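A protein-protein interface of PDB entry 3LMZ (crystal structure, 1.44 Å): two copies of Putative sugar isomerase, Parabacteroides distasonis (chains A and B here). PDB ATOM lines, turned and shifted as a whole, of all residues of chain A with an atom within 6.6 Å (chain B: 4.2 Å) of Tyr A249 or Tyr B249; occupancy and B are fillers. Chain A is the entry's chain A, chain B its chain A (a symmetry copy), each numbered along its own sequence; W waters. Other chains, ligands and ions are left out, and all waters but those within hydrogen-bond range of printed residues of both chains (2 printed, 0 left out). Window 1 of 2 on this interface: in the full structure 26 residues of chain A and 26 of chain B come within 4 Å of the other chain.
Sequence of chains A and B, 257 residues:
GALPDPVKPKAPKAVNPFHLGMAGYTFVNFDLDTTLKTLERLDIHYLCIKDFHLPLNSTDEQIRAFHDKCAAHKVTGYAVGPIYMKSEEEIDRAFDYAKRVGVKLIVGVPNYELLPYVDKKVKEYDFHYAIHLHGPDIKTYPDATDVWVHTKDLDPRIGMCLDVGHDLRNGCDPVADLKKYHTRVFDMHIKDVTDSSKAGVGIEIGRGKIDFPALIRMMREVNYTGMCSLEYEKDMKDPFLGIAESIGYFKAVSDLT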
ATOM      1  N   LYS A  10       7.295  13.383  -1.721  1.00  0.00           N
ATOM      2  CA  LYS A  10       6.528  13.780  -2.899  1.00  0.00           C
ATOM      3  C   LYS A  10       5.218  13.000  -2.987  1.00  0.00           C
ATOM      4  O   LYS A  10       5.020  12.007  -2.284  1.00  0.00           O
ATOM      5  CB  LYS A  10       7.345  13.577  -4.187  1.00  0.00           C
ATOM      6  CG  LYS A  10       7.611  12.121  -4.610  1.00  0.00           C
ATOM      7  CD  LYS A  10       8.482  12.012  -5.923  1.00  0.00           C
ATOM      8  CE  LYS A  10       8.636  10.600  -6.390  1.00  0.00           C
ATOM      9  NZ  LYS A  10       9.383  10.466  -7.695  1.00  0.00           N
ATOM     10  N   LYS A  13       2.797   8.256  -6.820  1.00  0.00           N
ATOM     11  CA  LYS A  13       2.508   8.145  -8.251  1.00  0.00           C
ATOM     12  C   LYS A  13       1.132   7.540  -8.491  1.00  0.00           C
ATOM     13  O   LYS A  13       0.719   6.627  -7.777  1.00  0.00           O
ATOM     14  CB  LYS A  13       3.538   7.314  -8.963  1.00  0.00           C
ATOM     15  CG  LYS A  13       4.907   7.956  -8.895  1.00  0.00           C
ATOM     16  CD  LYS A  13       6.008   7.147  -9.520  1.00  0.00           C
ATOM     17  CE  LYS A  13       7.301   7.905  -9.491  1.00  0.00           C
ATOM     18  NZ  LYS A  13       8.368   7.107 -10.113  1.00  0.00           N
ATOM     19  N   GLU A 204       9.491  13.440 -30.509  1.00  0.00           N
ATOM     20  CA  GLU A 204       9.608  12.986 -29.124  1.00  0.00           C
ATOM     21  C   GLU A 204       8.275  13.239 -28.428  1.00  0.00           C
ATOM     22  O   GLU A 204       7.695  14.291 -28.603  1.00  0.00           O
ATOM     23  CB  GLU A 204      10.735  13.771 -28.431  1.00  0.00           C
ATOM     24  CG  GLU A 204      12.095  13.439 -28.945  1.00  0.00           C
ATOM     25  CD  GLU A 204      12.569  14.269 -30.138  1.00  0.00           C
ATOM     26  OE1 GLU A 204      11.767  14.865 -30.899  1.00  0.00           O
ATOM     27  OE2 GLU A 204      13.824  14.326 -30.378  1.00  0.00           O
ATOM     28  N   ILE A 205       7.854  12.298 -27.567  1.00  0.00           N
ATOM     29  CA  ILE A 205       6.623  12.424 -26.827  1.00  0.00           C
ATOM     30  C   ILE A 205       6.693  13.668 -25.968  1.00  0.00           C
ATOM     31  O   ILE A 205       7.688  13.923 -25.254  1.00  0.00           O
ATOM     32  CB  ILE A 205       6.332  11.172 -25.965  1.00  0.00           C
ATOM     33  CG1 ILE A 205       5.924  10.027 -26.906  1.00  0.00           C
ATOM     34  CG2 ILE A 205       5.278  11.487 -24.881  1.00  0.00           C
ATOM     35  CD1 ILE A 205       5.560   8.742 -26.198  1.00  0.00           C
ATOM     36  N   GLY A 206       5.639  14.478 -26.079  1.00  0.00           N
ATOM     37  CA  GLY A 206       5.543  15.748 -25.382  1.00  0.00           C
ATOM     38  C   GLY A 206       5.777  16.953 -26.274  1.00  0.00           C
ATOM     39  O   GLY A 206       5.274  18.046 -25.969  1.00  0.00           O
ATOM     40  N   ARG A 207       6.567  16.763 -27.332  1.00  0.00           N
ATOM     41  CA  ARG A 207       6.886  17.834 -28.291  1.00  0.00           C
ATOM     42  C   ARG A 207       5.820  18.024 -29.352  1.00  0.00           C
ATOM     43  O   ARG A 207       5.851  19.022 -30.068  1.00  0.00           O
ATOM     44  CB  ARG A 207       8.238  17.610 -28.965  1.00  0.00           C
ATOM     45  CG  ARG A 207       9.363  17.567 -28.031  1.00  0.00           C
ATOM     46  CD  ARG A 207      10.671  17.607 -28.792  1.00  0.00           C
ATOM     47  NE  ARG A 207      11.882  17.262 -28.047  1.00  0.00           N
ATOM     48  CZ  ARG A 207      13.097  17.448 -28.500  1.00  0.00           C
ATOM     49  NH1 ARG A 207      13.297  18.112 -29.635  1.00  0.00           N
ATOM     50  NH2 ARG A 207      14.083  17.052 -27.774  1.00  0.00           N
ATOM     51  N   PHE A 212      -1.551  13.407 -24.292  1.00  0.00           N
ATOM     52  CA  PHE A 212      -1.265  12.292 -23.429  1.00  0.00           C
ATOM     53  C   PHE A 212      -2.050  12.283 -22.107  1.00  0.00           C
ATOM     54  O   PHE A 212      -2.520  11.216 -21.681  1.00  0.00           O
ATOM     55  CB  PHE A 212       0.271  12.117 -23.238  1.00  0.00           C
ATOM     56  CG  PHE A 212       0.943  11.496 -24.440  1.00  0.00           C
ATOM     57  CD1 PHE A 212       0.765  10.146 -24.713  1.00  0.00           C
ATOM     58  CD2 PHE A 212       1.586  12.285 -25.389  1.00  0.00           C
ATOM     59  CE1 PHE A 212       1.318   9.595 -25.904  1.00  0.00           C
ATOM     60  CE2 PHE A 212       2.152  11.733 -26.522  1.00  0.00           C
ATOM     61  CZ  PHE A 212       1.987  10.433 -26.801  1.00  0.00           C
ATOM     62  N   PRO A 213      -2.180  13.457 -21.419  1.00  0.00           N
ATOM     63  CA  PRO A 213      -2.999  13.442 -20.261  1.00  0.00           C
ATOM     64  C   PRO A 213      -4.421  12.907 -20.528  1.00  0.00           C
ATOM     65  O   PRO A 213      -4.951  12.122 -19.755  1.00  0.00           O
ATOM     66  CB  PRO A 213      -2.968  14.905 -19.822  1.00  0.00           C
ATOM     67  CG  PRO A 213      -1.676  15.371 -20.216  1.00  0.00           C
ATOM     68  CD  PRO A 213      -1.421  14.706 -21.555  1.00  0.00           C
ATOM     69  N   ALA A 244      14.470   7.753 -24.982  1.00  0.00           N
ATOM     70  CA  ALA A 244      14.551   7.990 -23.502  1.00  0.00           C
ATOM     71  C   ALA A 244      13.815   9.238 -23.071  1.00  0.00           C
ATOM     72  O   ALA A 244      13.066   9.202 -22.110  1.00  0.00           O
ATOM     73  CB  ALA A 244      16.038   8.076 -23.086  1.00  0.00           C
ATOM     74  N   GLU A 245      13.903  10.310 -23.885  1.00  0.00           N
ATOM     75  CA  GLU A 245      13.121  11.505 -23.574  1.00  0.00           C
ATOM     76  C   GLU A 245      11.634  11.201 -23.634  1.00  0.00           C
ATOM     77  O   GLU A 245      10.859  11.608 -22.776  1.00  0.00           O
ATOM     78  CB  GLU A 245      13.412  12.639 -24.567  1.00  0.00           C
ATOM     79  CG  GLU A 245      12.607  13.916 -24.298  1.00  0.00           C
ATOM     80  CD  GLU A 245      12.893  15.070 -25.257  1.00  0.00           C
ATOM     81  OE1 GLU A 245      13.979  15.022 -25.917  1.00  0.00           O
ATOM     82  OE2 GLU A 245      12.065  16.005 -25.261  1.00  0.00           O
ATOM     83  N   SER A 246      11.201  10.441 -24.656  1.00  0.00           N
ATOM     84  CA  SER A 246       9.798  10.142 -24.805  1.00  0.00           C
ATOM     85  C   SER A 246       9.282   9.310 -23.616  1.00  0.00           C
ATOM     86  O   SER A 246       8.147   9.533 -23.121  1.00  0.00           O
ATOM     87  CB  SER A 246       9.582   9.335 -26.072  1.00  0.00           C
ATOM     88  OG  SER A 246       9.847  10.031 -27.271  1.00  0.00           O
ATOM     89  N   ILE A 247      10.072   8.343 -23.148  1.00  0.00           N
ATOM     90  CA  ILE A 247       9.736   7.508 -22.017  1.00  0.00           C
ATOM     91  C   ILE A 247       9.641   8.361 -20.746  1.00  0.00           C
ATOM     92  O   ILE A 247       8.710   8.204 -19.921  1.00  0.00           O
ATOM     93  CB  ILE A 247      10.718   6.304 -21.904  1.00  0.00           C
ATOM     94  CG1 ILE A 247      10.490   5.305 -23.047  1.00  0.00           C
ATOM     95  CG2 ILE A 247      10.615   5.688 -20.510  1.00  0.00           C
ATOM     96  CD1 ILE A 247       9.102   4.668 -23.144  1.00  0.00           C
ATOM     97  N   GLY A 248      10.602   9.241 -20.538  1.00  0.00           N
ATOM     98  CA  GLY A 248      10.520  10.129 -19.387  1.00  0.00           C
ATOM     99  C   GLY A 248       9.287  10.988 -19.344  1.00  0.00           C
ATOM    100  O   GLY A 248       8.653  11.110 -18.342  1.00  0.00           O
ATOM    101  N   TYR A 249       8.957  11.597 -20.484  1.00  0.00           N
ATOM    102  CA  TYR A 249       7.794  12.440 -20.576  1.00  0.00           C
ATOM    103  C   TYR A 249       6.549  11.575 -20.262  1.00  0.00           C
ATOM    104  O   TYR A 249       5.663  11.915 -19.482  1.00  0.00           O
ATOM    105  CB  TYR A 249       7.682  13.124 -21.907  1.00  0.00           C
ATOM    106  CG  TYR A 249       6.771  14.343 -21.928  1.00  0.00           C
ATOM    107  CD1 TYR A 249       5.416  14.205 -21.970  1.00  0.00           C
ATOM    108  CD2 TYR A 249       7.308  15.640 -21.884  1.00  0.00           C
ATOM    109  CE1 TYR A 249       4.570  15.352 -21.920  1.00  0.00           C
ATOM    110  CE2 TYR A 249       6.503  16.744 -21.852  1.00  0.00           C
ATOM    111  CZ  TYR A 249       5.141  16.602 -21.860  1.00  0.00           C
ATOM    112  OH  TYR A 249       4.348  17.720 -21.809  1.00  0.00           O
ATOM    113  N   PHE A 250       6.424  10.405 -20.879  1.00  0.00           N
ATOM    114  CA  PHE A 250       5.258   9.552 -20.715  1.00  0.00           C
ATOM    115  C   PHE A 250       5.163   9.037 -19.283  1.00  0.00           C
ATOM    116  O   PHE A 250       4.046   8.899 -18.718  1.00  0.00           O
ATOM    117  CB  PHE A 250       5.318   8.368 -21.690  1.00  0.00           C
ATOM    118  CG  PHE A 250       4.062   7.532 -21.710  1.00  0.00           C
ATOM    119  CD1 PHE A 250       2.979   7.923 -22.448  1.00  0.00           C
ATOM    120  CD2 PHE A 250       3.976   6.395 -20.945  1.00  0.00           C
ATOM    121  CE1 PHE A 250       1.802   7.159 -22.461  1.00  0.00           C
ATOM    122  CE2 PHE A 250       2.797   5.646 -20.932  1.00  0.00           C
ATOM    123  CZ  PHE A 250       1.728   6.044 -21.673  1.00  0.00           C
ATOM    124  N   LYS A 251       6.295   8.692 -18.650  1.00  0.00           N
ATOM    125  CA  LYS A 251       6.250   8.252 -17.252  1.00  0.00           C
ATOM    126  C   LYS A 251       5.645   9.371 -16.365  1.00  0.00           C
ATOM    127  O   LYS A 251       4.809   9.138 -15.497  1.00  0.00           O
ATOM    128  CB  LYS A 251       7.628   7.880 -16.724  1.00  0.00           C
ATOM    129  CG  LYS A 251       8.157   6.527 -17.194  1.00  0.00           C
ATOM    130  CD  LYS A 251       9.586   6.305 -16.661  1.00  0.00           C
ATOM    131  CE  LYS A 251      10.155   4.955 -17.016  1.00  0.00           C
ATOM    132  NZ  LYS A 251      11.537   4.749 -16.406  1.00  0.00           N
ATOM    133  N   ALA A 252       6.108  10.600 -16.600  1.00  0.00           N
ATOM    134  CA  ALA A 252       5.592  11.715 -15.839  1.00  0.00           C
ATOM    135  C   ALA A 252       4.120  11.924 -16.042  1.00  0.00           C
ATOM    136  O   ALA A 252       3.403  12.113 -15.074  1.00  0.00           O
ATOM    137  CB  ALA A 252       6.356  13.013 -16.133  1.00  0.00           C
ATOM    138  N   VAL A 253       3.658  11.915 -17.294  1.00  0.00           N
ATOM    139  CA  VAL A 253       2.208  12.030 -17.538  1.00  0.00           C
ATOM    140  C   VAL A 253       1.437  10.919 -16.801  1.00  0.00           C
ATOM    141  O   VAL A 253       0.416  11.177 -16.167  1.00  0.00           O
ATOM    142  CB  VAL A 253       1.843  12.058 -19.023  1.00  0.00           C
ATOM    143  CG1 VAL A 253       0.301  12.163 -19.196  1.00  0.00           C
ATOM    144  CG2 VAL A 253       2.516  13.202 -19.706  1.00  0.00           C
ATOM    145  N   SER A 254       1.996   9.712 -16.813  1.00  0.00           N
ATOM    146  CA  SER A 254       1.338   8.533 -16.166  1.00  0.00           C
ATOM    147  C   SER A 254       1.232   8.738 -14.642  1.00  0.00           C
ATOM    148  O   SER A 254       0.239   8.373 -14.004  1.00  0.00           O
ATOM    149  CB  SER A 254       2.139   7.275 -16.433  1.00  0.00           C
ATOM    150  OG  SER A 254       2.157   7.000 -17.826  1.00  0.00           O
ATOM    151  N   ASP A 255       2.293   9.342 -14.088  1.00  0.00           N
ATOM    152  CA  ASP A 255       2.418   9.498 -12.650  1.00  0.00           C
ATOM    153  C   ASP A 255       1.567  10.635 -12.076  1.00  0.00           C
ATOM    154  O   ASP A 255       1.064  10.564 -10.924  1.00  0.00           O
ATOM    155  CB  ASP A 255       3.869   9.833 -12.256  1.00  0.00           C
ATOM    156  CG  ASP A 255       4.827   8.687 -12.432  1.00  0.00           C
ATOM    157  OD1 ASP A 255       4.387   7.530 -12.668  1.00  0.00           O
ATOM    158  OD2 ASP A 255       6.047   8.998 -12.374  1.00  0.00           O
ATOM    159  N   LEU A 256       1.435  11.723 -12.843  1.00  0.00           N
ATOM    160  CA  LEU A 256       0.949  13.018 -12.337  1.00  0.00           C
ATOM    161  C   LEU A 256      -0.460  13.361 -12.804  1.00  0.00           C
ATOM    162  O   LEU A 256      -1.086  14.306 -12.273  1.00  0.00           O
ATOM    163  CB  LEU A 256       1.934  14.123 -12.756  1.00  0.00           C
ATOM    164  CG  LEU A 256       3.369  14.031 -12.184  1.00  0.00           C
ATOM    165  CD1 LEU A 256       4.200  15.110 -12.817  1.00  0.00           C
ATOM    166  CD2 LEU A 256       3.415  14.124 -10.641  1.00  0.00           C
ATOM    167  N   ILE B 205      15.643  11.527 -13.092  1.00  0.00           N
ATOM    168  CA  ILE B 205      14.613  12.386 -12.562  1.00  0.00           C
ATOM    169  C   ILE B 205      13.275  11.692 -12.710  1.00  0.00           C
ATOM    170  O   ILE B 205      12.922  11.157 -13.785  1.00  0.00           O
ATOM    171  CB  ILE B 205      14.597  13.771 -13.253  1.00  0.00           C
ATOM    172  CG1 ILE B 205      15.827  14.558 -12.773  1.00  0.00           C
ATOM    173  CG2 ILE B 205      13.258  14.495 -12.993  1.00  0.00           C
ATOM    174  CD1 ILE B 205      15.921  15.959 -13.330  1.00  0.00           C
ATOM    175  N   GLY B 206      12.542  11.660 -11.596  1.00  0.00           N
ATOM    176  CA  GLY B 206      11.256  10.991 -11.518  1.00  0.00           C
ATOM    177  C   GLY B 206      11.302   9.664 -10.782  1.00  0.00           C
ATOM    178  O   GLY B 206      10.276   9.234 -10.230  1.00  0.00           O
ATOM    179  N   GLU B 245      16.039  10.712 -20.391  1.00  0.00           N
ATOM    180  CA  GLU B 245      14.858  10.371 -19.600  1.00  0.00           C
ATOM    181  C   GLU B 245      14.588  11.439 -18.554  1.00  0.00           C
ATOM    182  O   GLU B 245      13.457  11.860 -18.343  1.00  0.00           O
ATOM    183  CB  GLU B 245      15.039   9.032 -18.873  1.00  0.00           C
ATOM    184  CG  GLU B 245      13.835   8.628 -18.014  1.00  0.00           C
ATOM    185  CD  GLU B 245      13.978   7.289 -17.296  1.00  0.00           C
ATOM    186  OE1 GLU B 245      14.855   6.482 -17.738  1.00  0.00           O
ATOM    187  OE2 GLU B 245      13.167   7.067 -16.372  1.00  0.00           O
ATOM    188  N   SER B 246      15.647  11.927 -17.884  1.00  0.00           N
ATOM    189  CA  SER B 246      15.470  12.913 -16.848  1.00  0.00           C
ATOM    190  C   SER B 246      14.893  14.221 -17.424  1.00  0.00           C
ATOM    191  O   SER B 246      14.021  14.871 -16.792  1.00  0.00           O
ATOM    192  CB  SER B 246      16.811  13.232 -16.212  1.00  0.00           C
ATOM    193  OG  SER B 246      17.391  12.168 -15.487  1.00  0.00           O
ATOM    194  N   ILE B 247      15.364  14.640 -18.599  1.00  0.00           N
ATOM    195  CA  ILE B 247      14.892  15.826 -19.276  1.00  0.00           C
ATOM    196  C   ILE B 247      13.419  15.655 -19.668  1.00  0.00           C
ATOM    197  O   ILE B 247      12.587  16.579 -19.503  1.00  0.00           O
ATOM    198  CB  ILE B 247      15.827  16.197 -20.466  1.00  0.00           C
ATOM    199  CG1 ILE B 247      17.183  16.705 -19.956  1.00  0.00           C
ATOM    200  CG2 ILE B 247      15.109  17.169 -21.399  1.00  0.00           C
ATOM    201  CD1 ILE B 247      17.166  17.952 -19.070  1.00  0.00           C
ATOM    202  N   GLY B 248      13.071  14.507 -20.220  1.00  0.00           N
ATOM    203  CA  GLY B 248      11.671  14.264 -20.539  1.00  0.00           C
ATOM    204  C   GLY B 248      10.736  14.348 -19.365  1.00  0.00           C
ATOM    205  O   GLY B 248       9.709  14.949 -19.435  1.00  0.00           O
ATOM    206  N   TYR B 249      11.125  13.713 -18.259  1.00  0.00           N
ATOM    207  CA  TYR B 249      10.324  13.724 -17.064  1.00  0.00           C
ATOM    208  C   TYR B 249      10.179  15.194 -16.597  1.00  0.00           C
ATOM    209  O   TYR B 249       9.108  15.705 -16.279  1.00  0.00           O
ATOM    210  CB  TYR B 249      10.885  12.846 -15.985  1.00  0.00           C
ATOM    211  CG  TYR B 249       9.895  12.453 -14.897  1.00  0.00           C
ATOM    212  CD1 TYR B 249       9.559  13.327 -13.906  1.00  0.00           C
ATOM    213  CD2 TYR B 249       9.290  11.187 -14.902  1.00  0.00           C
ATOM    214  CE1 TYR B 249       8.580  12.973 -12.932  1.00  0.00           C
ATOM    215  CE2 TYR B 249       8.362  10.835 -13.962  1.00  0.00           C
ATOM    216  CZ  TYR B 249       8.001  11.726 -12.987  1.00  0.00           C
ATOM    217  OH  TYR B 249       7.055  11.365 -12.062  1.00  0.00           O
ATOM    218  N   PHE B 250      11.276  15.942 -16.526  1.00  0.00           N
ATOM    219  CA  PHE B 250      11.262  17.309 -16.028  1.00  0.00           C
ATOM    220  C   PHE B 250      10.460  18.214 -16.956  1.00  0.00           C
ATOM    221  O   PHE B 250       9.749  19.145 -16.496  1.00  0.00           O
ATOM    222  CB  PHE B 250      12.693  17.842 -15.890  1.00  0.00           C
ATOM    223  CG  PHE B 250      12.778  19.188 -15.213  1.00  0.00           C
ATOM    224  CD1 PHE B 250      12.746  19.283 -13.848  1.00  0.00           C
ATOM    225  CD2 PHE B 250      12.836  20.337 -15.962  1.00  0.00           C
ATOM    226  CE1 PHE B 250      12.809  20.531 -13.210  1.00  0.00           C
ATOM    227  CE2 PHE B 250      12.871  21.584 -15.332  1.00  0.00           C
ATOM    228  CZ  PHE B 250      12.841  21.664 -13.975  1.00  0.00           C
ATOM    229  N   LYS B 251      10.560  18.023 -18.281  1.00  0.00           N
ATOM    230  CA  LYS B 251       9.756  18.831 -19.202  1.00  0.00           C
ATOM    231  C   LYS B 251       8.247  18.631 -18.903  1.00  0.00           C
ATOM    232  O   LYS B 251       7.459  19.571 -18.859  1.00  0.00           O
ATOM    233  CB  LYS B 251      10.031  18.484 -20.658  1.00  0.00           C
ATOM    234  CG  LYS B 251      11.339  19.039 -21.219  1.00  0.00           C
ATOM    235  CD  LYS B 251      11.540  18.552 -22.668  1.00  0.00           C
ATOM    236  CE  LYS B 251      12.774  19.118 -23.324  1.00  0.00           C
ATOM    237  NZ  LYS B 251      12.893  18.670 -24.776  1.00  0.00           N
ATOM    238  N   ALA B 252       7.864  17.368 -18.713  1.00  0.00           N
ATOM    239  CA  ALA B 252       6.482  17.078 -18.409  1.00  0.00           C
ATOM    240  C   ALA B 252       6.028  17.707 -17.124  1.00  0.00           C
ATOM    241  O   ALA B 252       4.959  18.293 -17.090  1.00  0.00           O
ATOM    242  CB  ALA B 252       6.203  15.569 -18.387  1.00  0.00           C
ATOM    243  N   VAL B 253       6.814  17.574 -16.055  1.00  0.00           N
ATOM    244  CA  VAL B 253       6.452  18.247 -14.794  1.00  0.00           C
ATOM    245  C   VAL B 253       6.291  19.765 -15.007  1.00  0.00           C
ATOM    246  O   VAL B 253       5.332  20.367 -14.530  1.00  0.00           O
ATOM    247  CB  VAL B 253       7.424  17.956 -13.650  1.00  0.00           C
ATOM    248  CG1 VAL B 253       6.984  18.712 -12.364  1.00  0.00           C
ATOM    249  CG2 VAL B 253       7.494  16.489 -13.383  1.00  0.00           C
ATOM    250  N   ASP B 255       5.459  21.330 -17.735  1.00  0.00           N
ATOM    251  CA  ASP B 255       4.338  21.608 -18.613  1.00  0.00           C
ATOM    252  C   ASP B 255       2.971  21.435 -17.942  1.00  0.00           C
ATOM    253  O   ASP B 255       1.987  22.153 -18.259  1.00  0.00           O
ATOM    254  CB  ASP B 255       4.328  20.646 -19.816  1.00  0.00           C
ATOM    255  CG  ASP B 255       5.438  20.892 -20.800  1.00  0.00           C
ATOM    256  OD1 ASP B 255       6.139  21.937 -20.711  1.00  0.00           O
ATOM    257  OD2 ASP B 255       5.617  19.973 -21.644  1.00  0.00           O
HETATM  258  O   HOH W   1       9.935   7.661  -7.252  1.00  0.00           O
HETATM  259  O   HOH W   2       7.111  11.353  -9.261  1.00  0.00           O
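Lys B251 touches Arg A207 (NZ to NH2, 3.6 Å). Glu B245 touches Ala A244. Glu A245 touches Gly B248. Glu B245 touches Gly A248 (O to CA, 3.6 Å). Gly A248 touches Gly B248 (C to C, 3.7 Å). N of Tyr A249 touches N of Tyr B249, at 3.8 Å. Tyr A249 touches Ala B252 (CE2 to CA, 3.5 Å). Tyr B249 touches Lys A251 (CE2 to C, 3.9 Å). Ala A252 touches Tyr B249. Leu A256 touches Val B253.
Of the printed residues of chain B, Lys A13 touches Gly B206. Of chain B, only Gly B248 (3.4 Å), Tyr B249 (3.8 Å), Lys B251 (3.9 Å), Ala B252 (3.5 Å) and Asp B255 (2.6 Å) come within 4 Å of Tyr A249. Ser B246 touches none of the printed residues of chain A. Tyr B249 touches five residues of chain A. Of the printed residues of chain A, Ala B252 touches Tyr A249 (3.5 Å) and Ala A252 (3.4 Å). The nearest printed residue of chain B that does not touch Tyr A249 is Glu B245 (5.0 Å).
The side-chain carboxylate of Asp A255 lies within hydrogen-bond range of the side-chain hydroxyl of Tyr B249 (2.6 Å). NZ of Lys A10 is in hydrogen-bond range of O of Gly B206 (3.0 Å). O of Gly B206 lies within hydrogen-bond range of NZ of Lys A13, 2.9 Å away. NZ of Lys A251 lies within salt-bridge range of OE2 of Glu B245 (2.8 Å). NZ of Lys B251 lies within salt-bridge range of OE2 of Glu A245 (2.8 Å). OH of Tyr A249 sits at hydrogen-bond distance from OD2 of Asp B255, at 2.6 Å.
The side-chain amino group (NZ) of Lys A13 is in salt-bridge range of the side-chain carboxylate (OD2) of Asp A255. The side-chain carboxylate (OE1) of Glu A245 is in salt-bridge range of the guanidinium group (NH2) of Arg A207, 2.8 Å away. The guanidinium group (NE) of Arg A207 lies within salt-bridge range of the side-chain carboxylate (OE1) of Glu A204 (3.7 Å).
Water W2 lies within hydrogen-bond range of OH of Tyr B249 and NZ of Lys A10. Water W1 lies within hydrogen-bond range of NZ of Lys A10 (2.9 Å), NZ of Lys A13 (3.3 Å) and O of Gly B206 (3.4 Å).
Glu A245 touches Gly B248, and with the chains exchanged Gly A248 touches Glu B245. Glu A245 touches Lys B251, and with the chains exchanged Lys A251 touches Glu B245. Gly A248 touches Tyr B249, and with the chains exchanged Tyr A249 touches Gly B248. Ala B252 touches its own counterpart, Ala A252.
Printed residues of chain A that touch a printed residue of chain B: Lys A10, Lys A13, Arg A207, Ala A244, Glu A245, Gly A248, Tyr A249, Lys A251, Ala A252, Asp A255 and Leu A256. Hydrophobic or aromatic side chains of chain A that line the printed part of chain B: Ala A244, Tyr A249, Ala A252 and Leu A256. Of the 12 printed residues of chain B, 8 touch a printed residue of chain A. Printed residues of chain B that touch a printed residue of chain A: Gly B206, Glu B245, Gly B248, Tyr B249, Lys B251, Ala B252, Val B253 and Asp B255. Hydrophobic or aromatic side chains of chain B that line the printed part of chain A: Tyr B249, Ala B252 and Val B253. Among the printed residues, 20 pairs touch across the chains. Among the printed residues, Asp or Glu carboxylates within 4 Å of a Lys or Arg side-chain nitrogen of the other chain: Glu A245 with Lys B251 (2.8 Å) and Lys A251 with Glu B245 (2.8 Å).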
